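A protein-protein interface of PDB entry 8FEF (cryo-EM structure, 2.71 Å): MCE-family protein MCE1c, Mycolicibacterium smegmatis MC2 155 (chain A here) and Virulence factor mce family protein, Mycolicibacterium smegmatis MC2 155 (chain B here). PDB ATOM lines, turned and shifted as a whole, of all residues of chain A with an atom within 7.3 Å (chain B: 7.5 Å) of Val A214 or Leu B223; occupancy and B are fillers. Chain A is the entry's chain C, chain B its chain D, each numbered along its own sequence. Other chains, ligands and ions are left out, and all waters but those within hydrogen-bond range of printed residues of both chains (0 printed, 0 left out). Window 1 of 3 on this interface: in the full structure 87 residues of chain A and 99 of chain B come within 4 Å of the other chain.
The side-chain hydroxyl of Ser A211 lies close to the backbone carbonyl oxygen of Phe B219, 3.3 Å away.
The side-chain amide nitrogen (ND2) of Asn A215 lies within hydrogen-bond range of the backbone carbonyl oxygen (O) of Ala B222.
Among the printed residues, merely in contact across the chains: Ser A211 with Ala B222 (3.2 Å), Ser A211 with Leu B223 (3.2 Å), Asn A215 with Phe B230 (3.5 Å), Leu A218 with Phe B230 (3.6 Å), Ser A211 with Leu B218 (3.6 Å), Asn A215 with Leu B223 (3.6 Å), Leu A218 with Leu B233 (3.6 Å), Val A214 with Leu B223 (3.8 Å), Asn A215 with Ser B226 (3.8 Å) and Val A219 with Ser B226 (3.9 Å).
Gly A208 touches none of the printed residues of chain B.
Gln A213 touches none of the printed residues of chain B.
Val A214 touches just one residue of chain B: Leu B223.
Of the printed residues of chain A, Ala B222 touches Ser A211 (3.2 Å) and Asn A215 (2.5 Å).
Leu B223 touches three residues of chain A.
Of the printed residues of chain A, Ser B226 touches Asn A215 (3.8 Å) and Val A219 (3.9 Å).
Printed residues of chain A within 4 Å of Leu B233: Leu A218 (3.6 Å).
The nearest residue of chain A that does not touch Leu B223 is Leu A218 (4.1 Å).
The nearest printed residue of chain A that does not touch Phe B230 is Val A219 (4.7 Å).
Printed residues of chain B that touch a printed residue of chain A: Leu B218, Phe B219, Ala B222, Leu B223, Ser B226, Phe B230 and Leu B233.
Along chain B the printed residues that touch a printed residue of chain A span positions 218 to 233.
Hydrophobic or aromatic side chains of chain A that line the printed part of chain B: Val A214, Leu A218 and Val A219.
Among the printed residues, 12 pairs touch across the chains.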
ATOM      1  N   VAL A 206     -25.932  23.286  12.791  1.00  0.00           N
ATOM      2  CA  VAL A 206     -26.094  23.550  14.221  1.00  0.00           C
ATOM      3  C   VAL A 206     -25.628  22.353  15.044  1.00  0.00           C
ATOM      4  O   VAL A 206     -24.930  22.509  16.053  1.00  0.00           O
ATOM      5  CB  VAL A 206     -27.553  23.926  14.538  1.00  0.00           C
ATOM      6  CG1 VAL A 206     -27.759  24.035  16.039  1.00  0.00           C
ATOM      7  CG2 VAL A 206     -27.913  25.235  13.864  1.00  0.00           C
ATOM      8  N   LEU A 207     -26.003  21.142  14.624  1.00  0.00           N
ATOM      9  CA  LEU A 207     -25.600  19.941  15.356  1.00  0.00           C
ATOM     10  C   LEU A 207     -24.088  19.737  15.314  1.00  0.00           C
ATOM     11  O   LEU A 207     -23.464  19.434  16.337  1.00  0.00           O
ATOM     12  CB  LEU A 207     -26.315  18.714  14.792  1.00  0.00           C
ATOM     13  CG  LEU A 207     -27.747  18.461  15.262  1.00  0.00           C
ATOM     14  CD1 LEU A 207     -28.278  17.176  14.658  1.00  0.00           C
ATOM     15  CD2 LEU A 207     -27.807  18.407  16.777  1.00  0.00           C
ATOM     16  N   GLY A 208     -23.486  19.891  14.134  1.00  0.00           N
ATOM     17  CA  GLY A 208     -22.060  19.642  13.992  1.00  0.00           C
ATOM     18  C   GLY A 208     -21.203  20.646  14.736  1.00  0.00           C
ATOM     19  O   GLY A 208     -20.156  20.291  15.283  1.00  0.00           O
ATOM     20  N   ARG A 210     -21.917  22.022  17.494  1.00  0.00           N
ATOM     21  CA  ARG A 210     -22.066  21.756  18.919  1.00  0.00           C
ATOM     22  C   ARG A 210     -21.965  20.270  19.248  1.00  0.00           C
ATOM     23  O   ARG A 210     -22.460  19.838  20.292  1.00  0.00           O
ATOM     24  CB  ARG A 210     -23.398  22.315  19.419  1.00  0.00           C
ATOM     25  CG  ARG A 210     -23.613  23.782  19.101  1.00  0.00           C
ATOM     26  CD  ARG A 210     -22.541  24.645  19.736  1.00  0.00           C
ATOM     27  NE  ARG A 210     -22.759  26.061  19.473  1.00  0.00           N
ATOM     28  CZ  ARG A 210     -21.992  27.035  19.943  1.00  0.00           C
ATOM     29  NH1 ARG A 210     -20.940  26.780  20.703  1.00  0.00           N
ATOM     30  NH2 ARG A 210     -22.287  28.297  19.641  1.00  0.00           N
ATOM     31  N   SER A 211     -21.332  19.481  18.377  1.00  0.00           N
ATOM     32  CA  SER A 211     -21.284  18.034  18.576  1.00  0.00           C
ATOM     33  C   SER A 211     -20.469  17.653  19.807  1.00  0.00           C
ATOM     34  O   SER A 211     -20.842  16.728  20.541  1.00  0.00           O
ATOM     35  CB  SER A 211     -20.714  17.358  17.334  1.00  0.00           C
ATOM     36  OG  SER A 211     -20.666  15.960  17.526  1.00  0.00           O
ATOM     37  N   THR A 212     -19.345  18.335  20.035  1.00  0.00           N
ATOM     38  CA  THR A 212     -18.549  18.070  21.230  1.00  0.00           C
ATOM     39  C   THR A 212     -19.358  18.350  22.489  1.00  0.00           C
ATOM     40  O   THR A 212     -19.319  17.573  23.452  1.00  0.00           O
ATOM     41  CB  THR A 212     -17.272  18.911  21.207  1.00  0.00           C
ATOM     42  OG1 THR A 212     -16.517  18.605  20.030  1.00  0.00           O
ATOM     43  CG2 THR A 212     -16.418  18.625  22.431  1.00  0.00           C
ATOM     44  N   GLN A 213     -20.109  19.455  22.489  1.00  0.00           N
ATOM     45  CA  GLN A 213     -20.992  19.761  23.607  1.00  0.00           C
ATOM     46  C   GLN A 213     -22.049  18.680  23.782  1.00  0.00           C
ATOM     47  O   GLN A 213     -22.383  18.312  24.913  1.00  0.00           O
ATOM     48  CB  GLN A 213     -21.649  21.125  23.405  1.00  0.00           C
ATOM     49  CG  GLN A 213     -20.771  22.313  23.774  1.00  0.00           C
ATOM     50  CD  GLN A 213     -19.667  22.570  22.767  1.00  0.00           C
ATOM     51  OE1 GLN A 213     -19.676  22.028  21.663  1.00  0.00           O
ATOM     52  NE2 GLN A 213     -18.705  23.403  23.147  1.00  0.00           N
ATOM     53  N   VAL A 214     -22.588  18.159  22.675  1.00  0.00           N
ATOM     54  CA  VAL A 214     -23.603  17.111  22.757  1.00  0.00           C
ATOM     55  C   VAL A 214     -23.035  15.869  23.432  1.00  0.00           C
ATOM     56  O   VAL A 214     -23.634  15.315  24.361  1.00  0.00           O
ATOM     57  CB  VAL A 214     -24.160  16.788  21.359  1.00  0.00           C
ATOM     58  CG1 VAL A 214     -24.980  15.515  21.399  1.00  0.00           C
ATOM     59  CG2 VAL A 214     -25.011  17.935  20.852  1.00  0.00           C
ATOM     60  N   ASN A 215     -21.863  15.417  22.976  1.00  0.00           N
ATOM     61  CA  ASN A 215     -21.271  14.208  23.541  1.00  0.00           C
ATOM     62  C   ASN A 215     -20.906  14.407  25.008  1.00  0.00           C
ATOM     63  O   ASN A 215     -21.126  13.515  25.840  1.00  0.00           O
ATOM     64  CB  ASN A 215     -20.041  13.795  22.734  1.00  0.00           C
ATOM     65  CG  ASN A 215     -19.582  12.387  23.050  1.00  0.00           C
ATOM     66  OD1 ASN A 215     -20.297  11.617  23.689  1.00  0.00           O
ATOM     67  ND2 ASN A 215     -18.383  12.041  22.598  1.00  0.00           N
ATOM     68  N   GLN A 216     -20.344  15.572  25.340  1.00  0.00           N
ATOM     69  CA  GLN A 216     -19.970  15.847  26.721  1.00  0.00           C
ATOM     70  C   GLN A 216     -21.197  15.899  27.624  1.00  0.00           C
ATOM     71  O   GLN A 216     -21.176  15.369  28.742  1.00  0.00           O
ATOM     72  CB  GLN A 216     -19.182  17.154  26.794  1.00  0.00           C
ATOM     73  CG  GLN A 216     -18.452  17.373  28.101  1.00  0.00           C
ATOM     74  CD  GLN A 216     -17.440  18.495  28.011  1.00  0.00           C
ATOM     75  OE1 GLN A 216     -17.035  18.894  26.920  1.00  0.00           O
ATOM     76  NE2 GLN A 216     -17.025  19.011  29.161  1.00  0.00           N
ATOM     77  N   LEU A 217     -22.280  16.525  27.154  1.00  0.00           N
ATOM     78  CA  LEU A 217     -23.510  16.566  27.936  1.00  0.00           C
ATOM     79  C   LEU A 217     -24.079  15.168  28.135  1.00  0.00           C
ATOM     80  O   LEU A 217     -24.553  14.840  29.226  1.00  0.00           O
ATOM     81  CB  LEU A 217     -24.530  17.499  27.268  1.00  0.00           C
ATOM     82  CG  LEU A 217     -25.730  17.009  26.446  1.00  0.00           C
ATOM     83  CD1 LEU A 217     -26.956  16.771  27.311  1.00  0.00           C
ATOM     84  CD2 LEU A 217     -26.058  17.999  25.345  1.00  0.00           C
ATOM     85  N   LEU A 218     -24.029  14.325  27.099  1.00  0.00           N
ATOM     86  CA  LEU A 218     -24.557  12.969  27.233  1.00  0.00           C
ATOM     87  C   LEU A 218     -23.762  12.162  28.256  1.00  0.00           C
ATOM     88  O   LEU A 218     -24.343  11.504  29.131  1.00  0.00           O
ATOM     89  CB  LEU A 218     -24.565  12.269  25.874  1.00  0.00           C
ATOM     90  CG  LEU A 218     -25.587  12.792  24.862  1.00  0.00           C
ATOM     91  CD1 LEU A 218     -25.556  11.978  23.582  1.00  0.00           C
ATOM     92  CD2 LEU A 218     -26.980  12.796  25.461  1.00  0.00           C
ATOM     93  N   VAL A 219     -22.429  12.207  28.174  1.00  0.00           N
ATOM     94  CA  VAL A 219     -21.627  11.402  29.094  1.00  0.00           C
ATOM     95  C   VAL A 219     -21.735  11.937  30.520  1.00  0.00           C
ATOM     96  O   VAL A 219     -21.788  11.161  31.484  1.00  0.00           O
ATOM     97  CB  VAL A 219     -20.166  11.298  28.611  1.00  0.00           C
ATOM     98  CG1 VAL A 219     -20.110  10.631  27.245  1.00  0.00           C
ATOM     99  CG2 VAL A 219     -19.485  12.651  28.567  1.00  0.00           C
ATOM    100  N   ASN A 220     -21.793  13.264  30.684  1.00  0.00           N
ATOM    101  CA  ASN A 220     -21.936  13.824  32.023  1.00  0.00           C
ATOM    102  C   ASN A 220     -23.313  13.525  32.601  1.00  0.00           C
ATOM    103  O   ASN A 220     -23.449  13.314  33.811  1.00  0.00           O
ATOM    104  CB  ASN A 220     -21.670  15.327  31.997  1.00  0.00           C
ATOM    105  CG  ASN A 220     -20.235  15.653  31.654  1.00  0.00           C
ATOM    106  OD1 ASN A 220     -19.316  14.927  32.029  1.00  0.00           O
ATOM    107  ND2 ASN A 220     -20.034  16.751  30.940  1.00  0.00           N
ATOM    108  N   ALA B 217     -20.604  14.207   9.577  1.00  0.00           N
ATOM    109  CA  ALA B 217     -19.293  13.603   9.785  1.00  0.00           C
ATOM    110  C   ALA B 217     -18.686  14.065  11.098  1.00  0.00           C
ATOM    111  O   ALA B 217     -18.188  13.251  11.884  1.00  0.00           O
ATOM    112  CB  ALA B 217     -18.368  13.938   8.619  1.00  0.00           C
ATOM    113  N   LEU B 218     -18.727  15.375  11.359  1.00  0.00           N
ATOM    114  CA  LEU B 218     -18.227  15.868  12.642  1.00  0.00           C
ATOM    115  C   LEU B 218     -19.039  15.300  13.803  1.00  0.00           C
ATOM    116  O   LEU B 218     -18.475  14.904  14.835  1.00  0.00           O
ATOM    117  CB  LEU B 218     -18.241  17.398  12.676  1.00  0.00           C
ATOM    118  CG  LEU B 218     -17.007  18.165  12.191  1.00  0.00           C
ATOM    119  CD1 LEU B 218     -16.713  17.939  10.720  1.00  0.00           C
ATOM    120  CD2 LEU B 218     -17.171  19.648  12.480  1.00  0.00           C
ATOM    121  N   PHE B 219     -20.364  15.247  13.644  1.00  0.00           N
ATOM    122  CA  PHE B 219     -21.239  14.718  14.688  1.00  0.00           C
ATOM    123  C   PHE B 219     -20.867  13.284  15.053  1.00  0.00           C
ATOM    124  O   PHE B 219     -20.648  12.962  16.229  1.00  0.00           O
ATOM    125  CB  PHE B 219     -22.694  14.808  14.225  1.00  0.00           C
ATOM    126  CG  PHE B 219     -23.698  14.434  15.276  1.00  0.00           C
ATOM    127  CD1 PHE B 219     -23.960  15.286  16.336  1.00  0.00           C
ATOM    128  CD2 PHE B 219     -24.400  13.245  15.191  1.00  0.00           C
ATOM    129  CE1 PHE B 219     -24.889  14.949  17.299  1.00  0.00           C
ATOM    130  CE2 PHE B 219     -25.330  12.904  16.151  1.00  0.00           C
ATOM    131  CZ  PHE B 219     -25.576  13.757  17.204  1.00  0.00           C
ATOM    132  N   VAL B 220     -20.773  12.408  14.048  1.00  0.00           N
ATOM    133  CA  VAL B 220     -20.481  11.004  14.315  1.00  0.00           C
ATOM    134  C   VAL B 220     -19.049  10.836  14.813  1.00  0.00           C
ATOM    135  O   VAL B 220     -18.784  10.001  15.683  1.00  0.00           O
ATOM    136  CB  VAL B 220     -20.776  10.131  13.078  1.00  0.00           C
ATOM    137  CG1 VAL B 220     -22.243  10.238  12.696  1.00  0.00           C
ATOM    138  CG2 VAL B 220     -19.889  10.495  11.901  1.00  0.00           C
ATOM    139  N   ASN B 221     -18.104  11.623  14.285  1.00  0.00           N
ATOM    140  CA  ASN B 221     -16.724  11.518  14.745  1.00  0.00           C
ATOM    141  C   ASN B 221     -16.588  11.930  16.201  1.00  0.00           C
ATOM    142  O   ASN B 221     -15.678  11.460  16.892  1.00  0.00           O
ATOM    143  CB  ASN B 221     -15.805  12.368  13.868  1.00  0.00           C
ATOM    144  CG  ASN B 221     -15.593  11.769  12.497  1.00  0.00           C
ATOM    145  OD1 ASN B 221     -16.172  10.738  12.163  1.00  0.00           O
ATOM    146  ND2 ASN B 221     -14.763  12.417  11.691  1.00  0.00           N
ATOM    147  N   ALA B 222     -17.468  12.803  16.684  1.00  0.00           N
ATOM    148  CA  ALA B 222     -17.404  13.188  18.087  1.00  0.00           C
ATOM    149  C   ALA B 222     -18.216  12.278  19.000  1.00  0.00           C
ATOM    150  O   ALA B 222     -17.891  12.168  20.188  1.00  0.00           O
ATOM    151  CB  ALA B 222     -17.871  14.633  18.262  1.00  0.00           C
ATOM    152  N   LEU B 223     -19.261  11.619  18.493  1.00  0.00           N
ATOM    153  CA  LEU B 223     -20.151  10.838  19.349  1.00  0.00           C
ATOM    154  C   LEU B 223     -19.991   9.324  19.240  1.00  0.00           C
ATOM    155  O   LEU B 223     -20.643   8.602  20.000  1.00  0.00           O
ATOM    156  CB  LEU B 223     -21.615  11.201  19.071  1.00  0.00           C
ATOM    157  CG  LEU B 223     -22.243  12.294  19.936  1.00  0.00           C
ATOM    158  CD1 LEU B 223     -21.740  13.661  19.530  1.00  0.00           C
ATOM    159  CD2 LEU B 223     -23.756  12.229  19.864  1.00  0.00           C
ATOM    160  N   HIS B 224     -19.154   8.814  18.335  1.00  0.00           N
ATOM    161  CA  HIS B 224     -19.169   7.375  18.068  1.00  0.00           C
ATOM    162  C   HIS B 224     -18.487   6.547  19.150  1.00  0.00           C
ATOM    163  O   HIS B 224     -18.854   5.384  19.346  1.00  0.00           O
ATOM    164  CB  HIS B 224     -18.524   7.067  16.717  1.00  0.00           C
ATOM    165  CG  HIS B 224     -17.037   7.235  16.695  1.00  0.00           C
ATOM    166  ND1 HIS B 224     -16.202   6.361  16.033  1.00  0.00           N
ATOM    167  CD2 HIS B 224     -16.236   8.186  17.232  1.00  0.00           C
ATOM    168  CE1 HIS B 224     -14.950   6.758  16.176  1.00  0.00           C
ATOM    169  NE2 HIS B 224     -14.944   7.863  16.898  1.00  0.00           N
ATOM    170  N   ARG B 225     -17.501   7.104  19.855  1.00  0.00           N
ATOM    171  CA  ARG B 225     -16.729   6.287  20.787  1.00  0.00           C
ATOM    172  C   ARG B 225     -17.523   5.938  22.039  1.00  0.00           C
ATOM    173  O   ARG B 225     -17.325   4.863  22.615  1.00  0.00           O
ATOM    174  CB  ARG B 225     -15.434   7.004  21.164  1.00  0.00           C
ATOM    175  CG  ARG B 225     -14.373   6.945  20.082  1.00  0.00           C
ATOM    176  CD  ARG B 225     -13.096   7.652  20.502  1.00  0.00           C
ATOM    177  NE  ARG B 225     -12.043   7.483  19.509  1.00  0.00           N
ATOM    178  CZ  ARG B 225     -11.860   8.284  18.468  1.00  0.00           C
ATOM    179  NH1 ARG B 225     -12.639   9.333  18.258  1.00  0.00           N
ATOM    180  NH2 ARG B 225     -10.872   8.027  17.615  1.00  0.00           N
ATOM    181  N   SER B 226     -18.414   6.820  22.476  1.00  0.00           N
ATOM    182  CA  SER B 226     -19.113   6.650  23.749  1.00  0.00           C
ATOM    183  C   SER B 226     -20.482   6.005  23.538  1.00  0.00           C
ATOM    184  O   SER B 226     -21.512   6.544  23.928  1.00  0.00           O
ATOM    185  CB  SER B 226     -19.240   7.996  24.454  1.00  0.00           C
ATOM    186  OG  SER B 226     -17.974   8.614  24.604  1.00  0.00           O
ATOM    187  N   ASP B 227     -20.489   4.816  22.931  1.00  0.00           N
ATOM    188  CA  ASP B 227     -21.753   4.123  22.689  1.00  0.00           C
ATOM    189  C   ASP B 227     -22.234   3.369  23.923  1.00  0.00           C
ATOM    190  O   ASP B 227     -23.428   3.408  24.257  1.00  0.00           O
ATOM    191  CB  ASP B 227     -21.614   3.177  21.495  1.00  0.00           C
ATOM    192  CG  ASP B 227     -20.427   2.250  21.620  1.00  0.00           C
ATOM    193  OD1 ASP B 227     -19.416   2.658  22.227  1.00  0.00           O
ATOM    194  OD2 ASP B 227     -20.503   1.113  21.110  1.00  0.00           O
ATOM    195  N   PHE B 230     -23.793   5.762  26.074  1.00  0.00           N
ATOM    196  CA  PHE B 230     -25.171   6.095  25.718  1.00  0.00           C
ATOM    197  C   PHE B 230     -26.144   5.025  26.199  1.00  0.00           C
ATOM    198  O   PHE B 230     -27.245   5.346  26.668  1.00  0.00           O
ATOM    199  CB  PHE B 230     -25.303   6.292  24.208  1.00  0.00           C
ATOM    200  CG  PHE B 230     -24.429   7.379  23.651  1.00  0.00           C
ATOM    201  CD1 PHE B 230     -23.952   8.397  24.460  1.00  0.00           C
ATOM    202  CD2 PHE B 230     -24.083   7.379  22.312  1.00  0.00           C
ATOM    203  CE1 PHE B 230     -23.144   9.386  23.945  1.00  0.00           C
ATOM    204  CE2 PHE B 230     -23.280   8.369  21.791  1.00  0.00           C
ATOM    205  CZ  PHE B 230     -22.810   9.373  22.608  1.00  0.00           C
ATOM    206  N   LEU B 233     -26.514   5.554  29.778  1.00  0.00           N
ATOM    207  CA  LEU B 233     -27.324   6.746  30.008  1.00  0.00           C
ATOM    208  C   LEU B 233     -28.804   6.440  29.871  1.00  0.00           C
ATOM    209  O   LEU B 233     -29.614   6.888  30.688  1.00  0.00           O
ATOM    210  CB  LEU B 233     -26.917   7.851  29.035  1.00  0.00           C
ATOM    211  CG  LEU B 233     -27.838   9.068  28.945  1.00  0.00           C
ATOM    212  CD1 LEU B 233     -27.898   9.813  30.265  1.00  0.00           C
ATOM    213  CD2 LEU B 233     -27.388   9.986  27.829  1.00  0.00           C
